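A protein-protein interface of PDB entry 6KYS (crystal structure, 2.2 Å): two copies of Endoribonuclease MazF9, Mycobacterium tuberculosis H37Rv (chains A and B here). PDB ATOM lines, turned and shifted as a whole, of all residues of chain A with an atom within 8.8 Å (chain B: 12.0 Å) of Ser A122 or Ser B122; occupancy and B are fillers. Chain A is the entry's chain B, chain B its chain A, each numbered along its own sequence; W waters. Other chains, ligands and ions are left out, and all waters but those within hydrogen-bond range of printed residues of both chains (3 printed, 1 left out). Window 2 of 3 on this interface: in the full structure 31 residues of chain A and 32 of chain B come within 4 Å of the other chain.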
ATOM      1  N   ARG A   8      -9.564 -22.685 -32.384  1.00  0.00           N
ATOM      2  CA  ARG A   8     -10.140 -22.921 -31.063  1.00  0.00           C
ATOM      3  C   ARG A   8     -11.658 -23.058 -31.131  1.00  0.00           C
ATOM      4  O   ARG A   8     -12.339 -22.267 -31.789  1.00  0.00           O
ATOM      5  CB  ARG A   8      -9.756 -21.783 -30.110  1.00  0.00           C
ATOM      6  CG  ARG A   8      -9.852 -22.181 -28.635  1.00  0.00           C
ATOM      7  CD  ARG A   8      -9.346 -21.105 -27.681  1.00  0.00           C
ATOM      8  NE  ARG A   8      -9.123 -21.658 -26.348  1.00  0.00           N
ATOM      9  CZ  ARG A   8     -10.044 -21.699 -25.389  1.00  0.00           C
ATOM     10  NH1 ARG A   8     -11.255 -21.210 -25.611  1.00  0.00           N
ATOM     11  NH2 ARG A   8      -9.758 -22.235 -24.205  1.00  0.00           N
ATOM     12  N   LEU A 107     -18.278 -23.685 -25.384  1.00  0.00           N
ATOM     13  CA  LEU A 107     -16.854 -23.389 -25.253  1.00  0.00           C
ATOM     14  C   LEU A 107     -16.568 -22.618 -23.969  1.00  0.00           C
ATOM     15  O   LEU A 107     -15.530 -22.827 -23.332  1.00  0.00           O
ATOM     16  CB  LEU A 107     -16.347 -22.617 -26.473  1.00  0.00           C
ATOM     17  CG  LEU A 107     -14.844 -22.310 -26.492  1.00  0.00           C
ATOM     18  CD1 LEU A 107     -14.007 -23.586 -26.385  1.00  0.00           C
ATOM     19  CD2 LEU A 107     -14.454 -21.528 -27.739  1.00  0.00           C
ATOM     20  N   ALA A 108     -17.480 -21.726 -23.564  1.00  0.00           N
ATOM     21  CA  ALA A 108     -17.284 -21.019 -22.299  1.00  0.00           C
ATOM     22  C   ALA A 108     -17.332 -21.984 -21.117  1.00  0.00           C
ATOM     23  O   ALA A 108     -16.499 -21.905 -20.199  1.00  0.00           O
ATOM     24  CB  ALA A 108     -18.327 -19.910 -22.141  1.00  0.00           C
ATOM     25  N   GLN A 109     -18.290 -22.917 -21.129  1.00  0.00           N
ATOM     26  CA  GLN A 109     -18.300 -23.954 -20.102  1.00  0.00           C
ATOM     27  C   GLN A 109     -17.004 -24.759 -20.111  1.00  0.00           C
ATOM     28  O   GLN A 109     -16.507 -25.161 -19.053  1.00  0.00           O
ATOM     29  CB  GLN A 109     -19.501 -24.879 -20.293  1.00  0.00           C
ATOM     30  CG  GLN A 109     -20.846 -24.222 -20.074  1.00  0.00           C
ATOM     31  CD  GLN A 109     -21.991 -25.132 -20.469  1.00  0.00           C
ATOM     32  OE1 GLN A 109     -22.013 -25.668 -21.577  1.00  0.00           O
ATOM     33  NE2 GLN A 109     -22.943 -25.322 -19.563  1.00  0.00           N
ATOM     34  N   ASP A 111     -14.039 -23.609 -21.009  1.00  0.00           N
ATOM     35  CA  ASP A 111     -13.074 -22.734 -20.347  1.00  0.00           C
ATOM     36  C   ASP A 111     -13.156 -22.886 -18.834  1.00  0.00           C
ATOM     37  O   ASP A 111     -12.129 -23.028 -18.156  1.00  0.00           O
ATOM     38  CB  ASP A 111     -13.313 -21.274 -20.748  1.00  0.00           C
ATOM     39  CG  ASP A 111     -13.097 -21.017 -22.235  1.00  0.00           C
ATOM     40  OD1 ASP A 111     -12.507 -21.876 -22.931  1.00  0.00           O
ATOM     41  OD2 ASP A 111     -13.523 -19.944 -22.710  1.00  0.00           O
ATOM     42  N   GLU A 112     -14.377 -22.870 -18.285  1.00  0.00           N
ATOM     43  CA  GLU A 112     -14.521 -23.003 -16.835  1.00  0.00           C
ATOM     44  C   GLU A 112     -14.071 -24.380 -16.356  1.00  0.00           C
ATOM     45  O   GLU A 112     -13.454 -24.506 -15.291  1.00  0.00           O
ATOM     46  CB  GLU A 112     -15.966 -22.747 -16.403  1.00  0.00           C
ATOM     47  CG  GLU A 112     -16.468 -21.305 -16.543  1.00  0.00           C
ATOM     48  CD  GLU A 112     -15.510 -20.247 -16.003  1.00  0.00           C
ATOM     49  OE1 GLU A 112     -14.952 -20.416 -14.894  1.00  0.00           O
ATOM     50  OE2 GLU A 112     -15.344 -19.218 -16.688  1.00  0.00           O
ATOM     51  N   LYS A 115     -10.211 -24.334 -16.306  1.00  0.00           N
ATOM     52  CA  LYS A 115      -9.712 -23.580 -15.160  1.00  0.00           C
ATOM     53  C   LYS A 115      -9.898 -24.364 -13.870  1.00  0.00           C
ATOM     54  O   LYS A 115      -9.013 -24.381 -13.004  1.00  0.00           O
ATOM     55  CB  LYS A 115     -10.423 -22.234 -15.056  1.00  0.00           C
ATOM     56  CG  LYS A 115     -10.194 -21.310 -16.215  1.00  0.00           C
ATOM     57  CD  LYS A 115     -11.312 -20.303 -16.252  1.00  0.00           C
ATOM     58  CE  LYS A 115     -10.887 -18.989 -16.845  1.00  0.00           C
ATOM     59  NZ  LYS A 115     -12.008 -18.047 -16.651  1.00  0.00           N
ATOM     60  N   ASP A 119      -6.702 -25.825 -11.811  1.00  0.00           N
ATOM     61  CA  ASP A 119      -6.572 -25.022 -10.592  1.00  0.00           C
ATOM     62  C   ASP A 119      -6.121 -23.595 -10.902  1.00  0.00           C
ATOM     63  O   ASP A 119      -5.227 -23.046 -10.258  1.00  0.00           O
ATOM     64  CB  ASP A 119      -5.625 -25.702  -9.594  1.00  0.00           C
ATOM     65  CG  ASP A 119      -5.851 -25.238  -8.176  1.00  0.00           C
ATOM     66  OD1 ASP A 119      -6.862 -24.541  -7.942  1.00  0.00           O
ATOM     67  OD2 ASP A 119      -5.016 -25.555  -7.304  1.00  0.00           O
ATOM     68  N   LEU A 120      -6.756 -22.999 -11.908  1.00  0.00           N
ATOM     69  CA  LEU A 120      -6.458 -21.653 -12.372  1.00  0.00           C
ATOM     70  C   LEU A 120      -7.616 -20.724 -12.048  1.00  0.00           C
ATOM     71  O   LEU A 120      -8.773 -21.141 -12.033  1.00  0.00           O
ATOM     72  CB  LEU A 120      -6.181 -21.628 -13.885  1.00  0.00           C
ATOM     73  CG  LEU A 120      -5.236 -22.648 -14.526  1.00  0.00           C
ATOM     74  CD1 LEU A 120      -5.411 -22.647 -16.039  1.00  0.00           C
ATOM     75  CD2 LEU A 120      -3.799 -22.349 -14.164  1.00  0.00           C
ATOM     76  N   TRP A 121      -7.285 -19.458 -11.787  1.00  0.00           N
ATOM     77  CA  TRP A 121      -8.260 -18.401 -11.544  1.00  0.00           C
ATOM     78  C   TRP A 121      -7.899 -17.172 -12.372  1.00  0.00           C
ATOM     79  O   TRP A 121      -6.724 -16.892 -12.611  1.00  0.00           O
ATOM     80  CB  TRP A 121      -8.340 -18.030 -10.050  1.00  0.00           C
ATOM     81  N   SER A 122      -8.924 -16.442 -12.812  1.00  0.00           N
ATOM     82  CA  SER A 122      -8.726 -15.222 -13.598  1.00  0.00           C
ATOM     83  C   SER A 122      -9.774 -14.155 -13.243  1.00  0.00           C
ATOM     84  O   SER A 122      -9.469 -13.075 -12.712  1.00  0.00           O
ATOM     85  CB  SER A 122      -8.781 -15.533 -15.100  1.00  0.00           C
ATOM     86  OG  SER A 122      -7.514 -15.880 -15.628  1.00  0.00           O
ATOM     87  OXT SER A 122     -10.965 -14.384 -13.482  1.00  0.00           O
ATOM     88  N   ARG B   8       0.029 -31.008  -6.875  1.00  0.00           N
ATOM     89  CA  ARG B   8       0.274 -29.905  -7.788  1.00  0.00           C
ATOM     90  C   ARG B   8       1.561 -29.183  -7.406  1.00  0.00           C
ATOM     91  O   ARG B   8       1.772 -28.838  -6.241  1.00  0.00           O
ATOM     92  CB  ARG B   8      -0.916 -28.941  -7.756  1.00  0.00           C
ATOM     93  CG  ARG B   8      -0.983 -28.023  -8.961  1.00  0.00           C
ATOM     94  CD  ARG B   8      -2.242 -27.175  -8.997  1.00  0.00           C
ATOM     95  NE  ARG B   8      -2.405 -26.603 -10.329  1.00  0.00           N
ATOM     96  CZ  ARG B   8      -1.856 -25.462 -10.726  1.00  0.00           C
ATOM     97  NH1 ARG B   8      -1.120 -24.755  -9.884  1.00  0.00           N
ATOM     98  NH2 ARG B   8      -2.045 -25.027 -11.966  1.00  0.00           N
ATOM     99  N   ALA B 108       3.249 -20.036  -9.851  1.00  0.00           N
ATOM    100  CA  ALA B 108       2.355 -18.945 -10.234  1.00  0.00           C
ATOM    101  C   ALA B 108       2.599 -18.519 -11.677  1.00  0.00           C
ATOM    102  O   ALA B 108       1.651 -18.344 -12.458  1.00  0.00           O
ATOM    103  CB  ALA B 108       2.524 -17.758  -9.283  1.00  0.00           C
ATOM    104  N   GLN B 109       3.872 -18.365 -12.059  1.00  0.00           N
ATOM    105  CA  GLN B 109       4.140 -18.037 -13.458  1.00  0.00           C
ATOM    106  C   GLN B 109       3.721 -19.167 -14.393  1.00  0.00           C
ATOM    107  O   GLN B 109       3.363 -18.906 -15.546  1.00  0.00           O
ATOM    108  CB  GLN B 109       5.612 -17.675 -13.659  1.00  0.00           C
ATOM    109  CG  GLN B 109       5.976 -16.334 -13.055  1.00  0.00           C
ATOM    110  CD  GLN B 109       4.988 -15.250 -13.447  1.00  0.00           C
ATOM    111  OE1 GLN B 109       4.337 -14.650 -12.592  1.00  0.00           O
ATOM    112  NE2 GLN B 109       4.870 -14.994 -14.741  1.00  0.00           N
ATOM    113  N   LEU B 110       3.735 -20.419 -13.923  1.00  0.00           N
ATOM    114  CA  LEU B 110       3.238 -21.511 -14.760  1.00  0.00           C
ATOM    115  C   LEU B 110       1.718 -21.438 -14.934  1.00  0.00           C
ATOM    116  O   LEU B 110       1.208 -21.756 -16.013  1.00  0.00           O
ATOM    117  CB  LEU B 110       3.662 -22.863 -14.177  1.00  0.00           C
ATOM    118  CG  LEU B 110       3.296 -24.126 -14.977  1.00  0.00           C
ATOM    119  CD1 LEU B 110       3.818 -24.062 -16.411  1.00  0.00           C
ATOM    120  CD2 LEU B 110       3.804 -25.396 -14.280  1.00  0.00           C
ATOM    121  N   ASP B 111       0.984 -21.012 -13.898  1.00  0.00           N
ATOM    122  CA  ASP B 111      -0.438 -20.715 -14.066  1.00  0.00           C
ATOM    123  C   ASP B 111      -0.646 -19.639 -15.123  1.00  0.00           C
ATOM    124  O   ASP B 111      -1.563 -19.737 -15.948  1.00  0.00           O
ATOM    125  CB  ASP B 111      -1.060 -20.258 -12.743  1.00  0.00           C
ATOM    126  CG  ASP B 111      -0.993 -21.314 -11.653  1.00  0.00           C
ATOM    127  OD1 ASP B 111      -0.667 -22.479 -11.949  1.00  0.00           O
ATOM    128  OD2 ASP B 111      -1.273 -20.968 -10.489  1.00  0.00           O
ATOM    129  N   GLU B 112       0.193 -18.596 -15.103  1.00  0.00           N
ATOM    130  CA  GLU B 112       0.096 -17.552 -16.124  1.00  0.00           C
ATOM    131  C   GLU B 112       0.353 -18.113 -17.519  1.00  0.00           C
ATOM    132  O   GLU B 112      -0.366 -17.794 -18.476  1.00  0.00           O
ATOM    133  CB  GLU B 112       1.079 -16.424 -15.817  1.00  0.00           C
ATOM    134  CG  GLU B 112       0.694 -15.590 -14.618  1.00  0.00           C
ATOM    135  CD  GLU B 112      -0.735 -15.115 -14.695  1.00  0.00           C
ATOM    136  OE1 GLU B 112      -1.532 -15.490 -13.810  1.00  0.00           O
ATOM    137  OE2 GLU B 112      -1.062 -14.374 -15.648  1.00  0.00           O
ATOM    138  N   ALA B 113       1.398 -18.936 -17.656  1.00  0.00           N
ATOM    139  CA  ALA B 113       1.710 -19.529 -18.953  1.00  0.00           C
ATOM    140  C   ALA B 113       0.557 -20.386 -19.450  1.00  0.00           C
ATOM    141  O   ALA B 113       0.211 -20.343 -20.636  1.00  0.00           O
ATOM    142  CB  ALA B 113       2.993 -20.355 -18.863  1.00  0.00           C
ATOM    143  N   LEU B 114      -0.053 -21.163 -18.552  1.00  0.00           N
ATOM    144  CA  LEU B 114      -1.191 -21.998 -18.928  1.00  0.00           C
ATOM    145  C   LEU B 114      -2.365 -21.143 -19.397  1.00  0.00           C
ATOM    146  O   LEU B 114      -2.984 -21.429 -20.432  1.00  0.00           O
ATOM    147  CB  LEU B 114      -1.597 -22.892 -17.747  1.00  0.00           C
ATOM    148  CG  LEU B 114      -0.629 -24.022 -17.362  1.00  0.00           C
ATOM    149  CD1 LEU B 114      -1.030 -24.714 -16.069  1.00  0.00           C
ATOM    150  CD2 LEU B 114      -0.530 -25.044 -18.486  1.00  0.00           C
ATOM    151  N   LYS B 115      -2.681 -20.076 -18.651  1.00  0.00           N
ATOM    152  CA  LYS B 115      -3.772 -19.192 -19.061  1.00  0.00           C
ATOM    153  C   LYS B 115      -3.500 -18.562 -20.421  1.00  0.00           C
ATOM    154  O   LYS B 115      -4.415 -18.428 -21.245  1.00  0.00           O
ATOM    155  CB  LYS B 115      -3.999 -18.098 -18.021  1.00  0.00           C
ATOM    156  CG  LYS B 115      -4.589 -18.562 -16.710  1.00  0.00           C
ATOM    157  CD  LYS B 115      -4.802 -17.357 -15.823  1.00  0.00           C
ATOM    158  CE  LYS B 115      -4.030 -17.475 -14.534  1.00  0.00           C
ATOM    159  NZ  LYS B 115      -4.242 -16.282 -13.666  1.00  0.00           N
ATOM    160  N   LEU B 116      -2.252 -18.154 -20.670  1.00  0.00           N
ATOM    161  CA  LEU B 116      -1.898 -17.590 -21.968  1.00  0.00           C
ATOM    162  C   LEU B 116      -2.068 -18.617 -23.085  1.00  0.00           C
ATOM    163  O   LEU B 116      -2.742 -18.354 -24.088  1.00  0.00           O
ATOM    164  CB  LEU B 116      -0.460 -17.066 -21.933  1.00  0.00           C
ATOM    165  CG  LEU B 116       0.089 -16.510 -23.253  1.00  0.00           C
ATOM    166  CD1 LEU B 116      -0.748 -15.323 -23.725  1.00  0.00           C
ATOM    167  CD2 LEU B 116       1.561 -16.128 -23.149  1.00  0.00           C
ATOM    168  N   HIS B 117      -1.467 -19.801 -22.919  1.00  0.00           N
ATOM    169  CA  HIS B 117      -1.468 -20.808 -23.980  1.00  0.00           C
ATOM    170  C   HIS B 117      -2.874 -21.302 -24.295  1.00  0.00           C
ATOM    171  O   HIS B 117      -3.183 -21.607 -25.454  1.00  0.00           O
ATOM    172  CB  HIS B 117      -0.584 -21.993 -23.587  1.00  0.00           C
ATOM    173  CG  HIS B 117      -0.726 -23.178 -24.494  1.00  0.00           C
ATOM    174  ND1 HIS B 117      -0.243 -23.190 -25.787  1.00  0.00           N
ATOM    175  CD2 HIS B 117      -1.298 -24.390 -24.297  1.00  0.00           C
ATOM    176  CE1 HIS B 117      -0.514 -24.357 -26.346  1.00  0.00           C
ATOM    177  NE2 HIS B 117      -1.153 -25.103 -25.463  1.00  0.00           N
ATOM    178  N   LEU B 118      -3.729 -21.418 -23.278  1.00  0.00           N
ATOM    179  CA  LEU B 118      -5.071 -21.955 -23.458  1.00  0.00           C
ATOM    180  C   LEU B 118      -6.130 -20.868 -23.565  1.00  0.00           C
ATOM    181  O   LEU B 118      -7.324 -21.184 -23.636  1.00  0.00           O
ATOM    182  CB  LEU B 118      -5.416 -22.913 -22.315  1.00  0.00           C
ATOM    183  CG  LEU B 118      -4.553 -24.179 -22.184  1.00  0.00           C
ATOM    184  CD1 LEU B 118      -4.769 -24.859 -20.834  1.00  0.00           C
ATOM    185  CD2 LEU B 118      -4.839 -25.157 -23.324  1.00  0.00           C
ATOM    186  N   ASP B 119      -5.725 -19.600 -23.579  1.00  0.00           N
ATOM    187  CA  ASP B 119      -6.651 -18.486 -23.759  1.00  0.00           C
ATOM    188  C   ASP B 119      -7.739 -18.499 -22.685  1.00  0.00           C
ATOM    189  O   ASP B 119      -8.931 -18.340 -22.951  1.00  0.00           O
ATOM    190  CB  ASP B 119      -7.244 -18.498 -25.172  1.00  0.00           C
ATOM    191  CG  ASP B 119      -7.629 -17.122 -25.638  1.00  0.00           C
ATOM    192  OD1 ASP B 119      -7.649 -16.205 -24.794  1.00  0.00           O
ATOM    193  OD2 ASP B 119      -7.906 -16.955 -26.840  1.00  0.00           O
ATOM    194  N   LEU B 120      -7.303 -18.700 -21.448  1.00  0.00           N
ATOM    195  CA  LEU B 120      -8.215 -18.708 -20.318  1.00  0.00           C
ATOM    196  C   LEU B 120      -8.117 -17.400 -19.546  1.00  0.00           C
ATOM    197  O   LEU B 120      -7.756 -17.399 -18.368  1.00  0.00           O
ATOM    198  CB  LEU B 120      -7.926 -19.910 -19.417  1.00  0.00           C
ATOM    199  CG  LEU B 120      -7.998 -21.277 -20.103  1.00  0.00           C
ATOM    200  CD1 LEU B 120      -7.520 -22.402 -19.174  1.00  0.00           C
ATOM    201  CD2 LEU B 120      -9.421 -21.542 -20.596  1.00  0.00           C
ATOM    202  N   TRP B 121      -8.447 -16.282 -20.202  1.00  0.00           N
ATOM    203  CA  TRP B 121      -8.396 -14.971 -19.565  1.00  0.00           C
ATOM    204  C   TRP B 121      -9.684 -14.612 -18.835  1.00  0.00           C
ATOM    205  O   TRP B 121      -9.654 -13.706 -17.991  1.00  0.00           O
ATOM    206  CB  TRP B 121      -8.018 -13.928 -20.616  1.00  0.00           C
ATOM    207  CG  TRP B 121      -6.614 -14.157 -20.993  1.00  0.00           C
ATOM    208  CD1 TRP B 121      -6.129 -14.479 -22.225  1.00  0.00           C
ATOM    209  CD2 TRP B 121      -5.498 -14.151 -20.105  1.00  0.00           C
ATOM    210  NE1 TRP B 121      -4.770 -14.656 -22.162  1.00  0.00           N
ATOM    211  CE2 TRP B 121      -4.358 -14.457 -20.868  1.00  0.00           C
ATOM    212  CE3 TRP B 121      -5.352 -13.901 -18.734  1.00  0.00           C
ATOM    213  CZ2 TRP B 121      -3.085 -14.521 -20.309  1.00  0.00           C
ATOM    214  CZ3 TRP B 121      -4.094 -13.965 -18.178  1.00  0.00           C
ATOM    215  CH2 TRP B 121      -2.973 -14.274 -18.965  1.00  0.00           C
ATOM    216  N   SER B 122     -10.781 -15.313 -19.158  1.00  0.00           N
ATOM    217  CA  SER B 122     -12.059 -15.453 -18.416  1.00  0.00           C
ATOM    218  C   SER B 122     -13.221 -14.974 -19.266  1.00  0.00           C
ATOM    219  O   SER B 122     -13.053 -13.996 -20.005  1.00  0.00           O
ATOM    220  CB  SER B 122     -12.062 -14.744 -17.056  1.00  0.00           C
ATOM    221  OG  SER B 122     -11.597 -15.589 -16.018  1.00  0.00           O
ATOM    222  OXT SER B 122     -14.317 -15.550 -19.245  1.00  0.00           O
HETATM  223  O   HOH W   1      -4.141 -19.142 -11.856  1.00  0.00           O
HETATM  224  O   HOH W   2     -11.659 -18.173 -22.834  1.00  0.00           O
HETATM  225  O   HOH W   3     -14.996 -18.120 -21.251  1.00  0.00           O
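Printed residues of chain B within 4 Å of Arg A8: Leu B118 (2.7 Å), Asp B119 (3.9 Å) and Leu B120 (3.7 Å). Of the printed residues of chain B, Leu A120 touches Arg B8 (3.9 Å), Asp B111 (3.7 Å) and Leu B120 (3.8 Å). Of chain B, only Lys B115 comes within 4 Å of Trp A121. Of chain B, only Lys B115, Leu B120, Trp B121 and Ser B122 come within 4 Å of Ser A122. Ala B108 touches none of the printed residues of chain A. Of the printed residues of chain A, Asp B111 touches Leu A120 (3.7 Å). Glu B112 touches none of the printed residues of chain A. Of the printed residues of chain A, Trp B121 touches Ser A122 (3.5 Å). Of chain A, only Lys A115 and Ser A122 come within 4 Å of Ser B122.
Water W2 bridges the side-chain carboxylate of Asp A111 (2.6 Å) and the backbone carbonyl oxygen of Asp B119 (2.7 Å). Water W3 lies within hydrogen-bond range of the side-chain carboxylate of Asp A111 and the chain-end carboxylate of Ser B122. Water W1 bridges N of Trp A121 (3.2 Å) and NZ of Lys B115 (3.4 Å).
The side-chain amino group of Lys B115 is in hydrogen-bond range of the backbone carbonyl oxygen of Trp A121. The backbone carbonyl oxygen (O) of Leu B118 lies within hydrogen-bond range of the guanidinium group (NH2) of Arg A8, at 2.7 Å. O of Leu B120 lies within hydrogen-bond range of OG of Ser A122, at 3.1 Å. The side-chain hydroxyl (OG) of Ser B122 is in hydrogen-bond range of the side-chain amino group (NZ) of Lys A115. The chain-end carboxylate of Ser A122 sits at hydrogen-bond distance from the side-chain hydroxyl of Ser B122 (2.9 Å).
Hydrophobic or aromatic side chains of chain B within 4 Å of the printed part of chain A: Leu B120. Hydrophobic or aromatic side chains of chain A within 4 Å of the printed part of chain B: Leu A120. Among the printed residues, 15 pairs touch across the chains. Among the printed residues, no Asp or Glu carboxylate lies within 4 Å of a Lys or Arg side-chain nitrogen of the other chain.
Arg A8 touches Asp B119, and with the chains exchanged Asp A119 touches Arg B8. Lys A115 touches Leu B120, but with the chains exchanged Leu A120 does not touch Lys B115 (4.2 Å). Lys A115 touches Ser B122, and with the chains exchanged Ser A122 touches Lys B115. Ser A122 touches Leu B120, but with the chains exchanged Leu A120 does not touch Ser B122 (7.4 Å). 10 positions are printed for both chains. Of the 15 pairs that touch across the chains among the printed residues, 10 have their exchanged pair printed and touching as well.
Among the printed residues, merely in contact across the chains: Ser A122 with Lys B115 (3.1 Å), Asp A119 with Arg B8 (3.4 Å), Ser A122 with Trp B121 (3.5 Å), Arg A8 with Leu B120 (3.7 Å), Leu A120 with Asp B111 (3.7 Å), Leu A120 with Leu B120 (3.8 Å), Lys A115 with Leu B120 (3.8 Å), Asp A111 with Leu B120 (3.9 Å), Arg A8 with Asp B119 (3.9 Å) and Leu A120 with Arg B8 (3.9 Å).
The guanidinium group (NH2) of Arg B8 is in salt-bridge range of the side-chain carboxylate (OD1) of Asp B111 (2.9 Å). OE1 of Glu B112 is in salt-bridge range of NZ of Lys B115. The backbone carbonyl oxygen of Lys B115 sits at hydrogen-bond distance from the backbone NH of Leu B120. NH1 of Arg A8 lies within salt-bridge range of OD1 of Asp A111. NZ of Lys A115 lies within salt-bridge range of OE2 of Glu A112 (3.5 Å). The backbone carbonyl oxygen (O) of Lys A115 sits at hydrogen-bond distance from the backbone NH (N) of Leu A120, at 2.9 Å.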
